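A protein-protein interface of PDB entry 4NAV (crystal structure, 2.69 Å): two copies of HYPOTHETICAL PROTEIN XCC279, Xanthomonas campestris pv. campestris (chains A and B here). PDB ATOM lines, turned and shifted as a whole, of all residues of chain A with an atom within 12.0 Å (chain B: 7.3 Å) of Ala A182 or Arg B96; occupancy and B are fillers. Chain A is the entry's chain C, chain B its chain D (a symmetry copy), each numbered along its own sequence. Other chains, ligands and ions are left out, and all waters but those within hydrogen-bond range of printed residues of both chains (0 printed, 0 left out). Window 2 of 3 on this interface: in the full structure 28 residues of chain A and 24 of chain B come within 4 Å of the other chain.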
ATOM      1  N   VAL A 173      18.988  30.032  20.909  1.00  0.00           N
ATOM      2  CA  VAL A 173      18.985  28.569  20.942  1.00  0.00           C
ATOM      3  C   VAL A 173      17.709  28.029  21.517  1.00  0.00           C
ATOM      4  O   VAL A 173      17.066  27.170  20.892  1.00  0.00           O
ATOM      5  CB  VAL A 173      20.169  27.994  21.765  1.00  0.00           C
ATOM      6  CG1 VAL A 173      20.056  26.497  22.008  1.00  0.00           C
ATOM      7  CG2 VAL A 173      21.470  28.267  21.050  1.00  0.00           C
ATOM      8  N   ASP A 174      17.361  28.497  22.709  1.00  0.00           N
ATOM      9  CA  ASP A 174      16.178  28.004  23.415  1.00  0.00           C
ATOM     10  C   ASP A 174      14.972  27.977  22.510  1.00  0.00           C
ATOM     11  O   ASP A 174      14.197  27.029  22.546  1.00  0.00           O
ATOM     12  CB  ASP A 174      15.859  28.872  24.632  1.00  0.00           C
ATOM     13  CG  ASP A 174      16.702  28.528  25.847  1.00  0.00           C
ATOM     14  OD1 ASP A 174      17.653  27.732  25.736  1.00  0.00           O
ATOM     15  OD2 ASP A 174      16.395  29.050  26.934  1.00  0.00           O
ATOM     16  N   SER A 175      14.817  29.007  21.686  1.00  0.00           N
ATOM     17  CA  SER A 175      13.654  29.092  20.824  1.00  0.00           C
ATOM     18  C   SER A 175      13.804  28.189  19.599  1.00  0.00           C
ATOM     19  O   SER A 175      12.819  27.667  19.093  1.00  0.00           O
ATOM     20  CB  SER A 175      13.366  30.564  20.455  1.00  0.00           C
ATOM     21  OG  SER A 175      14.088  31.001  19.327  1.00  0.00           O
ATOM     22  N   ILE A 176      15.035  28.007  19.120  1.00  0.00           N
ATOM     23  CA  ILE A 176      15.285  27.069  18.018  1.00  0.00           C
ATOM     24  C   ILE A 176      14.821  25.709  18.436  1.00  0.00           C
ATOM     25  O   ILE A 176      14.017  25.087  17.751  1.00  0.00           O
ATOM     26  CB  ILE A 176      16.774  26.928  17.651  1.00  0.00           C
ATOM     27  N   ILE A 177      15.288  25.266  19.593  1.00  0.00           N
ATOM     28  CA  ILE A 177      14.869  23.975  20.131  1.00  0.00           C
ATOM     29  C   ILE A 177      13.366  23.849  20.357  1.00  0.00           C
ATOM     30  O   ILE A 177      12.762  22.827  20.050  1.00  0.00           O
ATOM     31  CB  ILE A 177      15.635  23.665  21.434  1.00  0.00           C
ATOM     32  CG1 ILE A 177      16.971  23.014  21.076  1.00  0.00           C
ATOM     33  CG2 ILE A 177      14.856  22.735  22.362  1.00  0.00           C
ATOM     34  CD1 ILE A 177      18.059  23.314  22.091  1.00  0.00           C
ATOM     35  N   ALA A 178      12.757  24.889  20.896  1.00  0.00           N
ATOM     36  CA  ALA A 178      11.318  24.870  21.129  1.00  0.00           C
ATOM     37  C   ALA A 178      10.551  24.719  19.816  1.00  0.00           C
ATOM     38  O   ALA A 178       9.542  24.002  19.771  1.00  0.00           O
ATOM     39  CB  ALA A 178      10.879  26.134  21.874  1.00  0.00           C
ATOM     40  N   ARG A 179      10.999  25.402  18.762  1.00  0.00           N
ATOM     41  CA  ARG A 179      10.288  25.353  17.489  1.00  0.00           C
ATOM     42  C   ARG A 179      10.261  23.925  16.980  1.00  0.00           C
ATOM     43  O   ARG A 179       9.273  23.498  16.406  1.00  0.00           O
ATOM     44  CB  ARG A 179      10.917  26.287  16.451  1.00  0.00           C
ATOM     45  N   PHE A 180      11.333  23.175  17.229  1.00  0.00           N
ATOM     46  CA  PHE A 180      11.448  21.814  16.680  1.00  0.00           C
ATOM     47  C   PHE A 180      11.042  20.664  17.606  1.00  0.00           C
ATOM     48  O   PHE A 180      11.134  19.499  17.210  1.00  0.00           O
ATOM     49  CB  PHE A 180      12.866  21.580  16.172  1.00  0.00           C
ATOM     50  CG  PHE A 180      13.141  22.256  14.865  1.00  0.00           C
ATOM     51  CD1 PHE A 180      12.602  21.755  13.691  1.00  0.00           C
ATOM     52  CD2 PHE A 180      13.890  23.411  14.809  1.00  0.00           C
ATOM     53  CE1 PHE A 180      12.837  22.371  12.480  1.00  0.00           C
ATOM     54  CE2 PHE A 180      14.118  24.038  13.602  1.00  0.00           C
ATOM     55  CZ  PHE A 180      13.608  23.506  12.429  1.00  0.00           C
ATOM     56  N   SER A 181      10.569  20.967  18.809  1.00  0.00           N
ATOM     57  CA  SER A 181      10.335  19.895  19.785  1.00  0.00           C
ATOM     58  C   SER A 181       9.005  19.203  19.629  1.00  0.00           C
ATOM     59  O   SER A 181       8.760  18.208  20.314  1.00  0.00           O
ATOM     60  CB  SER A 181      10.501  20.398  21.221  1.00  0.00           C
ATOM     61  OG  SER A 181      11.794  20.921  21.397  1.00  0.00           O
ATOM     62  N   ALA A 182       8.149  19.712  18.739  1.00  0.00           N
ATOM     63  CA  ALA A 182       6.918  18.981  18.361  1.00  0.00           C
ATOM     64  C   ALA A 182       6.263  19.650  17.162  1.00  0.00           C
ATOM     65  O   ALA A 182       6.169  19.053  16.101  1.00  0.00           O
ATOM     66  CB  ALA A 182       5.944  18.912  19.529  1.00  0.00           C
ATOM     67  N   ILE B  69      11.577   9.290   5.138  1.00  0.00           N
ATOM     68  CA  ILE B  69      10.850  10.527   5.378  1.00  0.00           C
ATOM     69  C   ILE B  69      11.796  11.696   5.284  1.00  0.00           C
ATOM     70  O   ILE B  69      12.725  11.822   6.075  1.00  0.00           O
ATOM     71  CB  ILE B  69      10.142  10.512   6.739  1.00  0.00           C
ATOM     72  CG1 ILE B  69       9.329   9.206   6.873  1.00  0.00           C
ATOM     73  CG2 ILE B  69       9.264  11.742   6.884  1.00  0.00           C
ATOM     74  CD1 ILE B  69       8.289   9.188   7.971  1.00  0.00           C
ATOM     75  N   VAL B  92       7.954  16.635   3.509  1.00  0.00           N
ATOM     76  CA  VAL B  92       7.128  16.619   4.704  1.00  0.00           C
ATOM     77  C   VAL B  92       7.442  17.828   5.600  1.00  0.00           C
ATOM     78  O   VAL B  92       8.601  18.045   6.000  1.00  0.00           O
ATOM     79  CB  VAL B  92       7.337  15.266   5.404  1.00  0.00           C
ATOM     80  CG1 VAL B  92       6.699  15.220   6.777  1.00  0.00           C
ATOM     81  CG2 VAL B  92       6.819  14.146   4.515  1.00  0.00           C
ATOM     82  N   LYS B  93       6.399  18.631   5.866  1.00  0.00           N
ATOM     83  CA  LYS B  93       6.511  19.832   6.699  1.00  0.00           C
ATOM     84  C   LYS B  93       6.742  19.415   8.162  1.00  0.00           C
ATOM     85  O   LYS B  93       7.603  19.979   8.837  1.00  0.00           O
ATOM     86  CB  LYS B  93       5.255  20.722   6.557  1.00  0.00           C
ATOM     87  N   ASN B  94       6.006  18.412   8.634  1.00  0.00           N
ATOM     88  CA  ASN B  94       6.201  17.901   9.996  1.00  0.00           C
ATOM     89  C   ASN B  94       6.307  16.376  10.054  1.00  0.00           C
ATOM     90  O   ASN B  94       5.365  15.661   9.690  1.00  0.00           O
ATOM     91  CB  ASN B  94       5.082  18.377  10.929  1.00  0.00           C
ATOM     92  CG  ASN B  94       5.223  17.814  12.329  1.00  0.00           C
ATOM     93  OD1 ASN B  94       5.091  16.605  12.523  1.00  0.00           O
ATOM     94  ND2 ASN B  94       5.517  18.666  13.304  1.00  0.00           N
ATOM     95  N   LYS B  95       7.430  15.888  10.567  1.00  0.00           N
ATOM     96  CA  LYS B  95       7.723  14.463  10.509  1.00  0.00           C
ATOM     97  C   LYS B  95       6.893  13.670  11.506  1.00  0.00           C
ATOM     98  O   LYS B  95       6.415  12.584  11.190  1.00  0.00           O
ATOM     99  CB  LYS B  95       9.214  14.215  10.663  1.00  0.00           C
ATOM    100  CG  LYS B  95      10.003  14.965   9.597  1.00  0.00           C
ATOM    101  CD  LYS B  95      11.348  14.334   9.301  1.00  0.00           C
ATOM    102  CE  LYS B  95      12.049  15.049   8.165  1.00  0.00           C
ATOM    103  NZ  LYS B  95      13.293  14.355   7.717  1.00  0.00           N
ATOM    104  N   ARG B  96       6.651  14.246  12.678  1.00  0.00           N
ATOM    105  CA  ARG B  96       5.713  13.638  13.626  1.00  0.00           C
ATOM    106  C   ARG B  96       4.389  13.313  12.951  1.00  0.00           C
ATOM    107  O   ARG B  96       3.951  12.178  12.987  1.00  0.00           O
ATOM    108  CB  ARG B  96       5.463  14.549  14.840  1.00  0.00           C
ATOM    109  CG  ARG B  96       4.766  13.848  15.991  1.00  0.00           C
ATOM    110  CD  ARG B  96       4.651  14.724  17.242  1.00  0.00           C
ATOM    111  NE  ARG B  96       3.419  15.490  17.390  1.00  0.00           N
ATOM    112  CZ  ARG B  96       3.232  16.725  16.934  1.00  0.00           C
ATOM    113  NH1 ARG B  96       4.185  17.361  16.259  1.00  0.00           N
ATOM    114  NH2 ARG B  96       2.075  17.325  17.141  1.00  0.00           N
ATOM    115  N   LEU B  97       3.758  14.316  12.331  1.00  0.00           N
ATOM    116  CA  LEU B  97       2.445  14.140  11.684  1.00  0.00           C
ATOM    117  C   LEU B  97       2.524  13.064  10.609  1.00  0.00           C
ATOM    118  O   LEU B  97       1.621  12.244  10.499  1.00  0.00           O
ATOM    119  CB  LEU B  97       1.910  15.455  11.120  1.00  0.00           C
ATOM    120  N   ALA B  98       3.621  13.032   9.852  1.00  0.00           N
ATOM    121  CA  ALA B  98       3.794  11.994   8.840  1.00  0.00           C
ATOM    122  C   ALA B  98       3.802  10.618   9.491  1.00  0.00           C
ATOM    123  O   ALA B  98       3.062   9.729   9.084  1.00  0.00           O
ATOM    124  CB  ALA B  98       5.066  12.218   8.068  1.00  0.00           C
ATOM    125  N   VAL B  99       4.638  10.456  10.514  1.00  0.00           N
ATOM    126  CA  VAL B  99       4.705   9.209  11.255  1.00  0.00           C
ATOM    127  C   VAL B  99       3.337   8.815  11.825  1.00  0.00           C
ATOM    128  O   VAL B  99       2.894   7.678  11.660  1.00  0.00           O
ATOM    129  CB  VAL B  99       5.752   9.290  12.391  1.00  0.00           C
ATOM    130  CG1 VAL B  99       5.613   8.125  13.352  1.00  0.00           C
ATOM    131  CG2 VAL B  99       7.165   9.294  11.822  1.00  0.00           C
ATOM    132  N   LEU B 100       2.683   9.757  12.494  1.00  0.00           N
ATOM    133  CA  LEU B 100       1.355   9.538  13.052  1.00  0.00           C
ATOM    134  C   LEU B 100       0.397   9.050  11.970  1.00  0.00           C
ATOM    135  O   LEU B 100      -0.465   8.241  12.223  1.00  0.00           O
ATOM    136  CB  LEU B 100       0.830  10.858  13.652  1.00  0.00           C
ATOM    137  CG  LEU B 100       0.362  11.064  15.087  1.00  0.00           C
ATOM    138  CD1 LEU B 100       1.232  10.336  16.087  1.00  0.00           C
ATOM    139  CD2 LEU B 100       0.340  12.566  15.403  1.00  0.00           C
ATOM    140  N   ALA B 101       0.535   9.556  10.752  1.00  0.00           N
ATOM    141  CA  ALA B 101      -0.345   9.152   9.658  1.00  0.00           C
ATOM    142  C   ALA B 101      -0.102   7.712   9.302  1.00  0.00           C
ATOM    143  O   ALA B 101      -1.041   6.952   9.080  1.00  0.00           O
ATOM    144  CB  ALA B 101      -0.124  10.040   8.436  1.00  0.00           C
ATOM    145  N   LEU B 102       1.170   7.344   9.262  1.00  0.00           N
ATOM    146  CA  LEU B 102       1.580   5.960   8.977  1.00  0.00           C
ATOM    147  C   LEU B 102       1.163   4.942  10.066  1.00  0.00           C
ATOM    148  O   LEU B 102       0.908   3.787   9.767  1.00  0.00           O
ATOM    149  CB  LEU B 102       3.088   5.891   8.790  1.00  0.00           C
ATOM    150  CG  LEU B 102       3.599   6.127   7.374  1.00  0.00           C
ATOM    151  CD1 LEU B 102       3.282   7.545   6.972  1.00  0.00           C
ATOM    152  CD2 LEU B 102       5.098   5.905   7.227  1.00  0.00           C
ATOM    153  N   LEU B 110       2.364   4.593  18.387  1.00  0.00           N
ATOM    154  CA  LEU B 110       3.703   5.183  18.385  1.00  0.00           C
ATOM    155  C   LEU B 110       4.733   4.319  19.100  1.00  0.00           C
ATOM    156  O   LEU B 110       5.926   4.315  18.722  1.00  0.00           O
ATOM    157  CB  LEU B 110       3.703   6.556  19.035  1.00  0.00           C
ATOM    158  CG  LEU B 110       3.031   7.657  18.205  1.00  0.00           C
ATOM    159  CD1 LEU B 110       2.949   8.961  19.011  1.00  0.00           C
ATOM    160  CD2 LEU B 110       3.743   7.851  16.865  1.00  0.00           C
ATOM    161  N   PHE B 115      12.346   5.461  14.830  1.00  0.00           N
ATOM    162  CA  PHE B 115      12.686   6.577  13.954  1.00  0.00           C
ATOM    163  C   PHE B 115      14.142   6.901  14.071  1.00  0.00           C
ATOM    164  O   PHE B 115      14.663   7.051  15.180  1.00  0.00           O
ATOM    165  CB  PHE B 115      11.874   7.824  14.297  1.00  0.00           C
ATOM    166  CG  PHE B 115      11.910   8.876  13.221  1.00  0.00           C
ATOM    167  CD1 PHE B 115      10.835   9.040  12.348  1.00  0.00           C
ATOM    168  CD2 PHE B 115      13.004   9.670  13.068  1.00  0.00           C
ATOM    169  CE1 PHE B 115      10.855   9.984  11.356  1.00  0.00           C
ATOM    170  CE2 PHE B 115      13.048  10.607  12.057  1.00  0.00           C
ATOM    171  CZ  PHE B 115      11.967  10.775  11.208  1.00  0.00           C
ATOM    172  N   PRO B 121      14.991  18.921  12.043  1.00  0.00           N
ATOM    173  CA  PRO B 121      13.668  18.563  11.498  1.00  0.00           C
ATOM    174  C   PRO B 121      13.132  17.173  11.946  1.00  0.00           C
ATOM    175  O   PRO B 121      11.928  16.964  11.911  1.00  0.00           O
ATOM    176  CB  PRO B 121      13.865  18.634   9.977  1.00  0.00           C
ATOM    177  CG  PRO B 121      15.146  19.411   9.787  1.00  0.00           C
ATOM    178  CD  PRO B 121      15.994  19.050  10.977  1.00  0.00           C
ATOM    179  N   ASP B 122      14.016  16.278  12.398  1.00  0.00           N
ATOM    180  CA  ASP B 122      13.629  14.953  12.884  1.00  0.00           C
ATOM    181  C   ASP B 122      13.153  14.955  14.347  1.00  0.00           C
ATOM    182  O   ASP B 122      12.572  13.986  14.839  1.00  0.00           O
ATOM    183  CB  ASP B 122      14.785  13.977  12.746  1.00  0.00           C
ATOM    184  CG  ASP B 122      15.382  13.962  11.345  1.00  0.00           C
ATOM    185  OD1 ASP B 122      14.668  13.682  10.364  1.00  0.00           O
ATOM    186  OD2 ASP B 122      16.597  14.243  11.216  1.00  0.00           O
ATOM    187  N   LEU B 123      13.366  16.057  15.036  1.00  0.00           N
ATOM    188  CA  LEU B 123      13.183  16.075  16.467  1.00  0.00           C
ATOM    189  C   LEU B 123      11.741  15.827  16.920  1.00  0.00           C
ATOM    190  O   LEU B 123      11.526  15.150  17.919  1.00  0.00           O
ATOM    191  CB  LEU B 123      13.714  17.387  17.031  1.00  0.00           C
ATOM    192  CG  LEU B 123      14.586  17.472  18.288  1.00  0.00           C
ATOM    193  CD1 LEU B 123      14.216  18.607  19.243  1.00  0.00           C
ATOM    194  CD2 LEU B 123      14.595  16.139  18.986  1.00  0.00           C
ATOM    195  N   PRO B 124      10.751  16.355  16.201  1.00  0.00           N
ATOM    196  CA  PRO B 124       9.381  16.117  16.621  1.00  0.00           C
ATOM    197  C   PRO B 124       9.037  14.645  16.671  1.00  0.00           C
ATOM    198  O   PRO B 124       8.386  14.170  17.610  1.00  0.00           O
ATOM    199  CB  PRO B 124       8.566  16.817  15.532  1.00  0.00           C
ATOM    200  CG  PRO B 124       9.441  17.931  15.050  1.00  0.00           C
ATOM    201  CD  PRO B 124      10.814  17.316  15.084  1.00  0.00           C
ATOM    202  N   ALA B 125       9.529  13.924  15.681  1.00  0.00           N
ATOM    203  CA  ALA B 125       9.350  12.490  15.594  1.00  0.00           C
ATOM    204  C   ALA B 125      10.218  11.760  16.620  1.00  0.00           C
ATOM    205  O   ALA B 125       9.750  10.850  17.318  1.00  0.00           O
ATOM    206  CB  ALA B 125       9.690  12.019  14.195  1.00  0.00           C
ATOM    207  N   LEU B 126      11.490  12.114  16.690  1.00  0.00           N
ATOM    208  CA  LEU B 126      12.365  11.452  17.636  1.00  0.00           C
ATOM    209  C   LEU B 126      11.766  11.491  19.028  1.00  0.00           C
ATOM    210  O   LEU B 126      11.828  10.478  19.765  1.00  0.00           O
ATOM    211  CB  LEU B 126      13.729  12.081  17.640  1.00  0.00           C
ATOM    212  CG  LEU B 126      14.549  11.726  16.397  1.00  0.00           C
ATOM    213  CD1 LEU B 126      15.688  12.702  16.169  1.00  0.00           C
ATOM    214  CD2 LEU B 126      15.092  10.306  16.532  1.00  0.00           C
ATOM    215  N   LEU B 127      11.118  12.604  19.389  1.00  0.00           N
ATOM    216  CA  LEU B 127      10.518  12.715  20.728  1.00  0.00           C
ATOM    217  C   LEU B 127       9.163  12.039  20.896  1.00  0.00           C
ATOM    218  O   LEU B 127       8.693  11.884  22.017  1.00  0.00           O
ATOM    219  CB  LEU B 127      10.394  14.176  21.147  1.00  0.00           C
ATOM    220  CG  LEU B 127      11.721  14.863  21.449  1.00  0.00           C
ATOM    221  CD1 LEU B 127      11.478  16.284  21.938  1.00  0.00           C
ATOM    222  CD2 LEU B 127      12.553  14.091  22.470  1.00  0.00           C
ATOM    223  N   ALA B 128       8.548  11.617  19.797  1.00  0.00           N
ATOM    224  CA  ALA B 128       7.225  11.002  19.842  1.00  0.00           C
ATOM    225  C   ALA B 128       7.231   9.451  19.729  1.00  0.00           C
ATOM    226  O   ALA B 128       6.308   8.801  20.200  1.00  0.00           O
ATOM    227  CB  ALA B 128       6.357  11.611  18.765  1.00  0.00           C
ATOM    228  N   VAL B 129       8.278   8.855  19.149  1.00  0.00           N
ATOM    229  CA  VAL B 129       8.252   7.407  18.876  1.00  0.00           C
ATOM    230  C   VAL B 129       8.731   6.518  20.033  1.00  0.00           C
ATOM    231  O   VAL B 129       9.400   6.967  20.948  1.00  0.00           O
ATOM    232  CB  VAL B 129       9.030   7.048  17.607  1.00  0.00           C
ATOM    233  CG1 VAL B 129       8.426   7.739  16.398  1.00  0.00           C
ATOM    234  CG2 VAL B 129      10.506   7.403  17.750  1.00  0.00           C
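Among the printed residues, merely in contact across the chains: Ala A182 with Pro B124, Phe A180 with Leu B123, Ser A181 with Leu B127 and Ser A181 with Leu B123.
Of the 23 printed residues of chain B, 5 touch a printed residue of chain A. Hydrophobic or aromatic side chains of chain B within 4 Å of the printed part of chain A: Leu B123, Pro B124 and Leu B127. Along chain B the printed residues that touch a printed residue of chain A span positions 94 to 127. Of the 10 printed residues of chain A, 3 touch a printed residue of chain B. Among the printed residues, 7 pairs touch across the chains. Among the printed residues, no Asp or Glu carboxylate lies within 4 Å of a Lys or Arg side-chain nitrogen of the other chain.
The backbone nitrogen (N) of Pro B124 lies close to the backbone carbonyl oxygen (O) of Phe A180. NH1 of Arg B96 lies within hydrogen-bond range of O of Ala A182, 2.6 Å away. The backbone carbonyl oxygen of Ala A182 is in hydrogen-bond range of the side-chain amide nitrogen of Asn B94 (2.9 Å).
No position is printed for both chains.
Of the printed residues of chain B, Ser A181 touches Leu B123 and Leu B127. Of chain B, only Asn B94 (2.9 Å), Arg B96 (2.6 Å) and Pro B124 (3.3 Å) come within 4 Å of Ala A182. Of chain A, only Ala A182 comes within 4 Å of Arg B96. No residue of chain A comes within 4 Å of Leu B97. Leu B102 touches none of the printed residues of chain A. Printed residues of chain A within 4 Å of Leu B123: Phe A180 (3.3 Å) and Ser A181 (3.98 Å). Pro B124 touches just these residues of chain A: Phe A180 and Ala A182. No residue of chain A comes within 4 Å of Ala B125. Of the printed residues of chain A, Leu B127 touches Ser A181. No residue of chain A comes within 4 Å of Ala B128. The nearest residue of chain B that does not touch Ala A182 is Leu B123 (5.6 Å). The nearest residue of chain A that does not touch Arg B96 is Ser A181 (6.2 Å). The nearest printed residue of chain B that does not touch Ser A181 is Pro B124 (4.3 Å).
The backbone carbonyl oxygen of Ile A177 lies within hydrogen-bond range of the side-chain hydroxyl of Ser A181 (2.5 Å). The side-chain amide oxygen of Asn B94 sits at hydrogen-bond distance from the backbone NH of Leu B97. The side-chain amide oxygen of Asn B94 sits at hydrogen-bond distance from the backbone NH of Arg B96, at 2.8 Å.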
